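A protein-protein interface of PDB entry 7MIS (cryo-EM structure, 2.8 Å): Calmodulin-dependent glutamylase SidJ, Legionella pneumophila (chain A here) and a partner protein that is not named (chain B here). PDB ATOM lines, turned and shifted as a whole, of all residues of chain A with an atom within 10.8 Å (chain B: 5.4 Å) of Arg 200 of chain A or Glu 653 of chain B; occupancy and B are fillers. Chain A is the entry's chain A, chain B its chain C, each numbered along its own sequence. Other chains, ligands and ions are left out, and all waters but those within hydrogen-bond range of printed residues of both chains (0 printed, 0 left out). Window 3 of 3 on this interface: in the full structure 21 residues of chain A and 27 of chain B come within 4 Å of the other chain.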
ATOM      1  N   HIS A 139      22.705 -17.836 -10.187  1.00  0.00           N
ATOM      2  CA  HIS A 139      21.754 -18.515 -11.057  1.00  0.00           C
ATOM      3  C   HIS A 139      21.895 -20.031 -11.018  1.00  0.00           C
ATOM      4  O   HIS A 139      21.054 -20.725 -11.596  1.00  0.00           O
ATOM      5  CB  HIS A 139      21.920 -18.027 -12.493  1.00  0.00           C
ATOM      6  CG  HIS A 139      21.663 -16.565 -12.668  1.00  0.00           C
ATOM      7  ND1 HIS A 139      20.982 -15.813 -11.737  1.00  0.00           N
ATOM      8  CD2 HIS A 139      21.999 -15.713 -13.664  1.00  0.00           C
ATOM      9  CE1 HIS A 139      20.908 -14.562 -12.151  1.00  0.00           C
ATOM     10  NE2 HIS A 139      21.518 -14.475 -13.319  1.00  0.00           N
ATOM     11  N   ARG A 167      12.868 -22.819  -7.618  1.00  0.00           N
ATOM     12  CA  ARG A 167      13.960 -23.562  -8.233  1.00  0.00           C
ATOM     13  C   ARG A 167      15.016 -22.670  -8.876  1.00  0.00           C
ATOM     14  O   ARG A 167      16.052 -23.182  -9.308  1.00  0.00           O
ATOM     15  CB  ARG A 167      13.412 -24.522  -9.293  1.00  0.00           C
ATOM     16  CG  ARG A 167      12.632 -23.842 -10.402  1.00  0.00           C
ATOM     17  CD  ARG A 167      12.444 -24.760 -11.599  1.00  0.00           C
ATOM     18  NE  ARG A 167      11.324 -25.675 -11.412  1.00  0.00           N
ATOM     19  CZ  ARG A 167      11.424 -26.900 -10.915  1.00  0.00           C
ATOM     20  NH1 ARG A 167      12.589 -27.405 -10.542  1.00  0.00           N
ATOM     21  NH2 ARG A 167      10.326 -27.639 -10.788  1.00  0.00           N
ATOM     22  N   ASP A 168      14.788 -21.358  -8.947  1.00  0.00           N
ATOM     23  CA  ASP A 168      15.692 -20.494  -9.698  1.00  0.00           C
ATOM     24  C   ASP A 168      17.071 -20.414  -9.053  1.00  0.00           C
ATOM     25  O   ASP A 168      18.085 -20.386  -9.756  1.00  0.00           O
ATOM     26  CB  ASP A 168      15.091 -19.097  -9.831  1.00  0.00           C
ATOM     27  CG  ASP A 168      14.030 -19.020 -10.903  1.00  0.00           C
ATOM     28  OD1 ASP A 168      14.292 -19.483 -12.031  1.00  0.00           O
ATOM     29  OD2 ASP A 168      12.934 -18.494 -10.620  1.00  0.00           O
ATOM     30  N   PHE A 197      18.078 -15.278 -16.157  1.00  0.00           N
ATOM     31  CA  PHE A 197      19.019 -16.165 -16.824  1.00  0.00           C
ATOM     32  C   PHE A 197      18.359 -16.797 -18.037  1.00  0.00           C
ATOM     33  O   PHE A 197      17.145 -17.000 -18.074  1.00  0.00           O
ATOM     34  CB  PHE A 197      19.577 -17.246 -15.879  1.00  0.00           C
ATOM     35  CG  PHE A 197      18.576 -18.275 -15.457  1.00  0.00           C
ATOM     36  CD1 PHE A 197      17.850 -18.113 -14.293  1.00  0.00           C
ATOM     37  CD2 PHE A 197      18.389 -19.423 -16.203  1.00  0.00           C
ATOM     38  CE1 PHE A 197      16.939 -19.064 -13.896  1.00  0.00           C
ATOM     39  CE2 PHE A 197      17.478 -20.376 -15.811  1.00  0.00           C
ATOM     40  CZ  PHE A 197      16.753 -20.198 -14.655  1.00  0.00           C
ATOM     41  N   ARG A 198      19.180 -17.105 -19.031  1.00  0.00           N
ATOM     42  CA  ARG A 198      18.701 -17.510 -20.347  1.00  0.00           C
ATOM     43  C   ARG A 198      18.906 -19.013 -20.494  1.00  0.00           C
ATOM     44  O   ARG A 198      19.952 -19.474 -20.950  1.00  0.00           O
ATOM     45  CB  ARG A 198      19.431 -16.729 -21.429  1.00  0.00           C
ATOM     46  CG  ARG A 198      18.679 -16.626 -22.729  1.00  0.00           C
ATOM     47  CD  ARG A 198      19.636 -16.643 -23.895  1.00  0.00           C
ATOM     48  NE  ARG A 198      20.494 -15.465 -23.931  1.00  0.00           N
ATOM     49  CZ  ARG A 198      20.129 -14.283 -24.410  1.00  0.00           C
ATOM     50  NH1 ARG A 198      18.916 -14.077 -24.897  1.00  0.00           N
ATOM     51  NH2 ARG A 198      21.005 -13.283 -24.402  1.00  0.00           N
ATOM     52  N   GLU A 199      17.893 -19.782 -20.106  1.00  0.00           N
ATOM     53  CA  GLU A 199      17.923 -21.214 -20.348  1.00  0.00           C
ATOM     54  C   GLU A 199      17.829 -21.482 -21.850  1.00  0.00           C
ATOM     55  O   GLU A 199      17.714 -20.569 -22.672  1.00  0.00           O
ATOM     56  CB  GLU A 199      16.811 -21.916 -19.568  1.00  0.00           C
ATOM     57  CG  GLU A 199      15.393 -21.632 -20.039  1.00  0.00           C
ATOM     58  CD  GLU A 199      14.822 -20.365 -19.435  1.00  0.00           C
ATOM     59  OE1 GLU A 199      15.607 -19.556 -18.898  1.00  0.00           O
ATOM     60  OE2 GLU A 199      13.590 -20.176 -19.494  1.00  0.00           O
ATOM     61  N   ARG A 200      17.878 -22.764 -22.214  1.00  0.00           N
ATOM     62  CA  ARG A 200      18.058 -23.124 -23.617  1.00  0.00           C
ATOM     63  C   ARG A 200      16.913 -22.608 -24.481  1.00  0.00           C
ATOM     64  O   ARG A 200      17.139 -22.113 -25.590  1.00  0.00           O
ATOM     65  CB  ARG A 200      18.193 -24.639 -23.749  1.00  0.00           C
ATOM     66  CG  ARG A 200      19.312 -25.220 -22.896  1.00  0.00           C
ATOM     67  CD  ARG A 200      19.820 -26.545 -23.435  1.00  0.00           C
ATOM     68  NE  ARG A 200      21.198 -26.795 -23.027  1.00  0.00           N
ATOM     69  CZ  ARG A 200      22.066 -27.532 -23.709  1.00  0.00           C
ATOM     70  NH1 ARG A 200      21.733 -28.124 -24.844  1.00  0.00           N
ATOM     71  NH2 ARG A 200      23.302 -27.678 -23.239  1.00  0.00           N
ATOM     72  N   LEU A 201      15.677 -22.714 -23.993  1.00  0.00           N
ATOM     73  CA  LEU A 201      14.527 -22.336 -24.809  1.00  0.00           C
ATOM     74  C   LEU A 201      14.298 -20.828 -24.798  1.00  0.00           C
ATOM     75  O   LEU A 201      14.362 -20.174 -25.844  1.00  0.00           O
ATOM     76  CB  LEU A 201      13.277 -23.072 -24.325  1.00  0.00           C
ATOM     77  CG  LEU A 201      13.023 -24.442 -24.960  1.00  0.00           C
ATOM     78  CD1 LEU A 201      12.639 -24.301 -26.422  1.00  0.00           C
ATOM     79  CD2 LEU A 201      14.241 -25.341 -24.817  1.00  0.00           C
ATOM     80  N   SER A 202      14.036 -20.256 -23.623  1.00  0.00           N
ATOM     81  CA  SER A 202      13.681 -18.848 -23.508  1.00  0.00           C
ATOM     82  C   SER A 202      14.462 -18.224 -22.359  1.00  0.00           C
ATOM     83  O   SER A 202      15.331 -18.856 -21.752  1.00  0.00           O
ATOM     84  CB  SER A 202      12.170 -18.681 -23.304  1.00  0.00           C
ATOM     85  OG  SER A 202      11.711 -19.485 -22.232  1.00  0.00           O
ATOM     86  N   THR A 203      14.150 -16.964 -22.069  1.00  0.00           N
ATOM     87  CA  THR A 203      14.757 -16.229 -20.970  1.00  0.00           C
ATOM     88  C   THR A 203      13.814 -16.224 -19.777  1.00  0.00           C
ATOM     89  O   THR A 203      12.618 -15.955 -19.922  1.00  0.00           O
ATOM     90  CB  THR A 203      15.077 -14.791 -21.384  1.00  0.00           C
ATOM     91  OG1 THR A 203      15.783 -14.794 -22.630  1.00  0.00           O
ATOM     92  CG2 THR A 203      15.926 -14.102 -20.327  1.00  0.00           C
ATOM     93  N   ASN A 204      14.353 -16.525 -18.598  1.00  0.00           N
ATOM     94  CA  ASN A 204      13.587 -16.575 -17.362  1.00  0.00           C
ATOM     95  C   ASN A 204      13.936 -15.351 -16.528  1.00  0.00           C
ATOM     96  O   ASN A 204      15.088 -15.189 -16.100  1.00  0.00           O
ATOM     97  CB  ASN A 204      13.883 -17.863 -16.598  1.00  0.00           C
ATOM     98  CG  ASN A 204      13.159 -17.933 -15.272  1.00  0.00           C
ATOM     99  OD1 ASN A 204      12.152 -17.261 -15.065  1.00  0.00           O
ATOM    100  ND2 ASN A 204      13.671 -18.751 -14.363  1.00  0.00           N
ATOM    101  N   PRO A 611      14.751 -10.872 -25.255  1.00  0.00           N
ATOM    102  CA  PRO A 611      13.790 -11.185 -26.318  1.00  0.00           C
ATOM    103  C   PRO A 611      12.907  -9.987 -26.637  1.00  0.00           C
ATOM    104  O   PRO A 611      12.527  -9.217 -25.755  1.00  0.00           O
ATOM    105  CB  PRO A 611      12.978 -12.346 -25.733  1.00  0.00           C
ATOM    106  CG  PRO A 611      13.172 -12.245 -24.262  1.00  0.00           C
ATOM    107  CD  PRO A 611      14.561 -11.735 -24.079  1.00  0.00           C
ATOM    108  N   LYS B   7      22.870 -27.265 -32.603  1.00  0.00           N
ATOM    109  CA  LYS B   7      22.810 -26.281 -31.535  1.00  0.00           C
ATOM    110  C   LYS B   7      23.051 -24.890 -32.106  1.00  0.00           C
ATOM    111  O   LYS B   7      23.841 -24.710 -33.036  1.00  0.00           O
ATOM    112  CB  LYS B   7      23.832 -26.596 -30.434  1.00  0.00           C
ATOM    113  CG  LYS B   7      23.848 -25.604 -29.282  1.00  0.00           C
ATOM    114  CD  LYS B   7      22.578 -25.679 -28.455  1.00  0.00           C
ATOM    115  CE  LYS B   7      22.555 -24.594 -27.393  1.00  0.00           C
ATOM    116  NZ  LYS B   7      22.434 -23.238 -27.997  1.00  0.00           N
ATOM    117  N   ASN B  11      22.199 -17.827 -28.058  1.00  0.00           N
ATOM    118  CA  ASN B  11      21.648 -17.646 -26.725  1.00  0.00           C
ATOM    119  C   ASN B  11      22.708 -17.570 -25.639  1.00  0.00           C
ATOM    120  O   ASN B  11      22.412 -17.080 -24.545  1.00  0.00           O
ATOM    121  CB  ASN B  11      20.677 -18.792 -26.394  1.00  0.00           C
ATOM    122  CG  ASN B  11      21.347 -20.152 -26.418  1.00  0.00           C
ATOM    123  OD1 ASN B  11      22.572 -20.255 -26.464  1.00  0.00           O
ATOM    124  ND2 ASN B  11      20.541 -21.206 -26.385  1.00  0.00           N
ATOM    125  N   PRO B 100      29.545 -28.573 -26.635  1.00  0.00           N
ATOM    126  CA  PRO B 100      29.046 -27.189 -26.716  1.00  0.00           C
ATOM    127  C   PRO B 100      29.871 -26.184 -25.931  1.00  0.00           C
ATOM    128  O   PRO B 100      30.010 -25.037 -26.372  1.00  0.00           O
ATOM    129  CB  PRO B 100      27.618 -27.306 -26.166  1.00  0.00           C
ATOM    130  CG  PRO B 100      27.242 -28.719 -26.391  1.00  0.00           C
ATOM    131  CD  PRO B 100      28.495 -29.507 -26.198  1.00  0.00           C
ATOM    132  N   THR B 651      15.472 -30.950 -28.072  1.00  0.00           N
ATOM    133  CA  THR B 651      16.246 -30.399 -26.971  1.00  0.00           C
ATOM    134  C   THR B 651      15.951 -31.188 -25.704  1.00  0.00           C
ATOM    135  O   THR B 651      14.846 -31.700 -25.518  1.00  0.00           O
ATOM    136  CB  THR B 651      15.917 -28.914 -26.751  1.00  0.00           C
ATOM    137  OG1 THR B 651      16.343 -28.151 -27.886  1.00  0.00           O
ATOM    138  CG2 THR B 651      16.605 -28.383 -25.507  1.00  0.00           C
ATOM    139  N   LEU B 652      16.951 -31.289 -24.837  1.00  0.00           N
ATOM    140  CA  LEU B 652      16.806 -31.924 -23.531  1.00  0.00           C
ATOM    141  C   LEU B 652      16.953 -30.831 -22.478  1.00  0.00           C
ATOM    142  O   LEU B 652      18.070 -30.451 -22.118  1.00  0.00           O
ATOM    143  CB  LEU B 652      17.835 -33.034 -23.345  1.00  0.00           C
ATOM    144  CG  LEU B 652      17.801 -33.741 -21.988  1.00  0.00           C
ATOM    145  CD1 LEU B 652      18.009 -35.234 -22.159  1.00  0.00           C
ATOM    146  CD2 LEU B 652      18.841 -33.161 -21.036  1.00  0.00           C
ATOM    147  N   GLU B 653      15.821 -30.313 -22.002  1.00  0.00           N
ATOM    148  CA  GLU B 653      15.807 -29.211 -21.040  1.00  0.00           C
ATOM    149  C   GLU B 653      15.544 -29.757 -19.640  1.00  0.00           C
ATOM    150  O   GLU B 653      14.444 -29.663 -19.097  1.00  0.00           O
ATOM    151  CB  GLU B 653      14.771 -28.167 -21.442  1.00  0.00           C
ATOM    152  CG  GLU B 653      14.721 -26.963 -20.514  1.00  0.00           C
ATOM    153  CD  GLU B 653      16.004 -26.156 -20.541  1.00  0.00           C
ATOM    154  OE1 GLU B 653      16.712 -26.202 -21.566  1.00  0.00           O
ATOM    155  OE2 GLU B 653      16.308 -25.485 -19.535  1.00  0.00           O
ATOM    156  N   GLY B 654      16.587 -30.332 -19.045  1.00  0.00           N
ATOM    157  CA  GLY B 654      16.511 -30.734 -17.654  1.00  0.00           C
ATOM    158  C   GLY B 654      15.694 -32.001 -17.447  1.00  0.00           C
ATOM    159  O   GLY B 654      15.633 -32.884 -18.303  1.00  0.00           O
ATOM    160  N   LYS B 655      15.063 -32.079 -16.277  1.00  0.00           N
ATOM    161  CA  LYS B 655      14.295 -33.248 -15.877  1.00  0.00           C
ATOM    162  C   LYS B 655      13.029 -32.797 -15.164  1.00  0.00           C
ATOM    163  O   LYS B 655      12.941 -31.675 -14.659  1.00  0.00           O
ATOM    164  CB  LYS B 655      15.109 -34.170 -14.959  1.00  0.00           C
ATOM    165  CG  LYS B 655      16.311 -34.815 -15.625  1.00  0.00           C
ATOM    166  CD  LYS B 655      17.386 -35.153 -14.609  1.00  0.00           C
ATOM    167  CE  LYS B 655      18.426 -36.092 -15.192  1.00  0.00           C
ATOM    168  NZ  LYS B 655      19.380 -36.581 -14.160  1.00  0.00           N
ATOM    169  N   ARG B 662      13.387 -34.651 -19.571  1.00  0.00           N
ATOM    170  CA  ARG B 662      12.377 -33.845 -20.239  1.00  0.00           C
ATOM    171  C   ARG B 662      12.870 -33.496 -21.635  1.00  0.00           C
ATOM    172  O   ARG B 662      13.965 -32.948 -21.789  1.00  0.00           O
ATOM    173  CB  ARG B 662      12.085 -32.572 -19.443  1.00  0.00           C
ATOM    174  CG  ARG B 662      10.975 -31.713 -20.019  1.00  0.00           C
ATOM    175  CD  ARG B 662      10.911 -30.369 -19.326  1.00  0.00           C
ATOM    176  NE  ARG B 662      10.163 -30.439 -18.076  1.00  0.00           N
ATOM    177  CZ  ARG B 662      10.470 -29.773 -16.970  1.00  0.00           C
ATOM    178  NH1 ARG B 662      11.516 -28.963 -16.913  1.00  0.00           N
ATOM    179  NH2 ARG B 662       9.706 -29.921 -15.892  1.00  0.00           N
ATOM    180  N   TYR B 663      12.066 -33.815 -22.644  1.00  0.00           N
ATOM    181  CA  TYR B 663      12.418 -33.587 -24.037  1.00  0.00           C
ATOM    182  C   TYR B 663      11.443 -32.603 -24.662  1.00  0.00           C
ATOM    183  O   TYR B 663      10.235 -32.671 -24.418  1.00  0.00           O
ATOM    184  CB  TYR B 663      12.410 -34.894 -24.829  1.00  0.00           C
ATOM    185  CG  TYR B 663      13.699 -35.669 -24.739  1.00  0.00           C
ATOM    186  CD1 TYR B 663      14.834 -35.244 -25.414  1.00  0.00           C
ATOM    187  CD2 TYR B 663      13.785 -36.828 -23.982  1.00  0.00           C
ATOM    188  CE1 TYR B 663      16.015 -35.949 -25.337  1.00  0.00           C
ATOM    189  CE2 TYR B 663      14.961 -37.539 -23.900  1.00  0.00           C
ATOM    190  CZ  TYR B 663      16.074 -37.096 -24.578  1.00  0.00           C
ATOM    191  OH  TYR B 663      17.251 -37.802 -24.496  1.00  0.00           O
ATOM    192  N   ILE B 664      11.974 -31.686 -25.465  1.00  0.00           N
ATOM    193  CA  ILE B 664      11.185 -30.688 -26.176  1.00  0.00           C
ATOM    194  C   ILE B 664      11.437 -30.875 -27.662  1.00  0.00           C
ATOM    195  O   ILE B 664      12.588 -30.837 -28.111  1.00  0.00           O
ATOM    196  CB  ILE B 664      11.543 -29.259 -25.739  1.00  0.00           C
ATOM    197  CG1 ILE B 664      11.288 -29.076 -24.246  1.00  0.00           C
ATOM    198  CG2 ILE B 664      10.736 -28.243 -26.527  1.00  0.00           C
ATOM    199  CD1 ILE B 664      12.299 -28.193 -23.583  1.00  0.00           C
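NE of Arg 198 of chain A lies within hydrogen-bond range of O of Asn 11 of chain B (2.6 Å).
The backbone NH (N) of Glu 653 of chain B is in hydrogen-bond range of the backbone carbonyl oxygen (O) of Arg 662 of chain B (3.2 Å). OE2 of Glu 199 of chain A lies within hydrogen-bond range of OG of Ser 202 of chain A, at 3.4 Å. NZ of Lys 7 of chain B sits close to ND2 of Asn 11 of chain B. N of Asn 204 of chain A is in hydrogen-bond range of OE1 of Glu 199 of chain A (3.3 Å). The backbone NH (N) of Ile 664 of chain B lies within hydrogen-bond range of the backbone carbonyl oxygen (O) of Thr 651 of chain B, 2.9 Å away.
Among the printed residues, pairs that only touch across the chains: Arg 200 of chain A with Glu 653 of chain B (3.1 Å), Glu 199 of chain A with Glu 653 of chain B (3.6 Å), Arg 200 of chain A with Asn 11 of chain B (3.6 Å), Leu 201 of chain A with Ile 664 of chain B (3.7 Å) and Leu 201 of chain A with Thr 651 of chain B (3.9 Å).
Of the printed residues of chain B, Arg 198 of chain A touches Asn 11 (2.6 Å). Of the printed residues of chain B, Glu 199 of chain A touches Glu 653 (3.6 Å). Arg 200 of chain A touches just these residues of chain B: Asn 11 and Glu 653. Of the printed residues of chain B, Leu 201 of chain A touches Thr 651 (3.9 Å) and Ile 664 (3.7 Å). Of the printed residues of chain A, Asn 11 of chain B touches Arg 198 (2.6 Å) and Arg 200 (3.6 Å). No residue of chain A comes within 4 Å of Leu 652 of chain B. Glu 653 of chain B touches just these residues of chain A: Glu 199 and Arg 200. No residue of chain A comes within 4 Å of Gly 654 of chain B. Of the printed residues of chain A, Ile 664 of chain B touches Leu 201.
Of the 12 printed residues of chain A, 4 touch a printed residue of chain B. Printed residues of chain A that touch a printed residue of chain B: Arg 198, Glu 199, Arg 200 and Leu 201. Hydrophobic or aromatic side chains of chain A that line the printed part of chain B: Leu 201. Printed residues of chain B that touch a printed residue of chain A: Asn 11, Thr 651, Glu 653 and Ile 664. Among the printed residues, no Asp or Glu carboxylate lies within 4 Å of a Lys or Arg side-chain nitrogen of the other chain.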
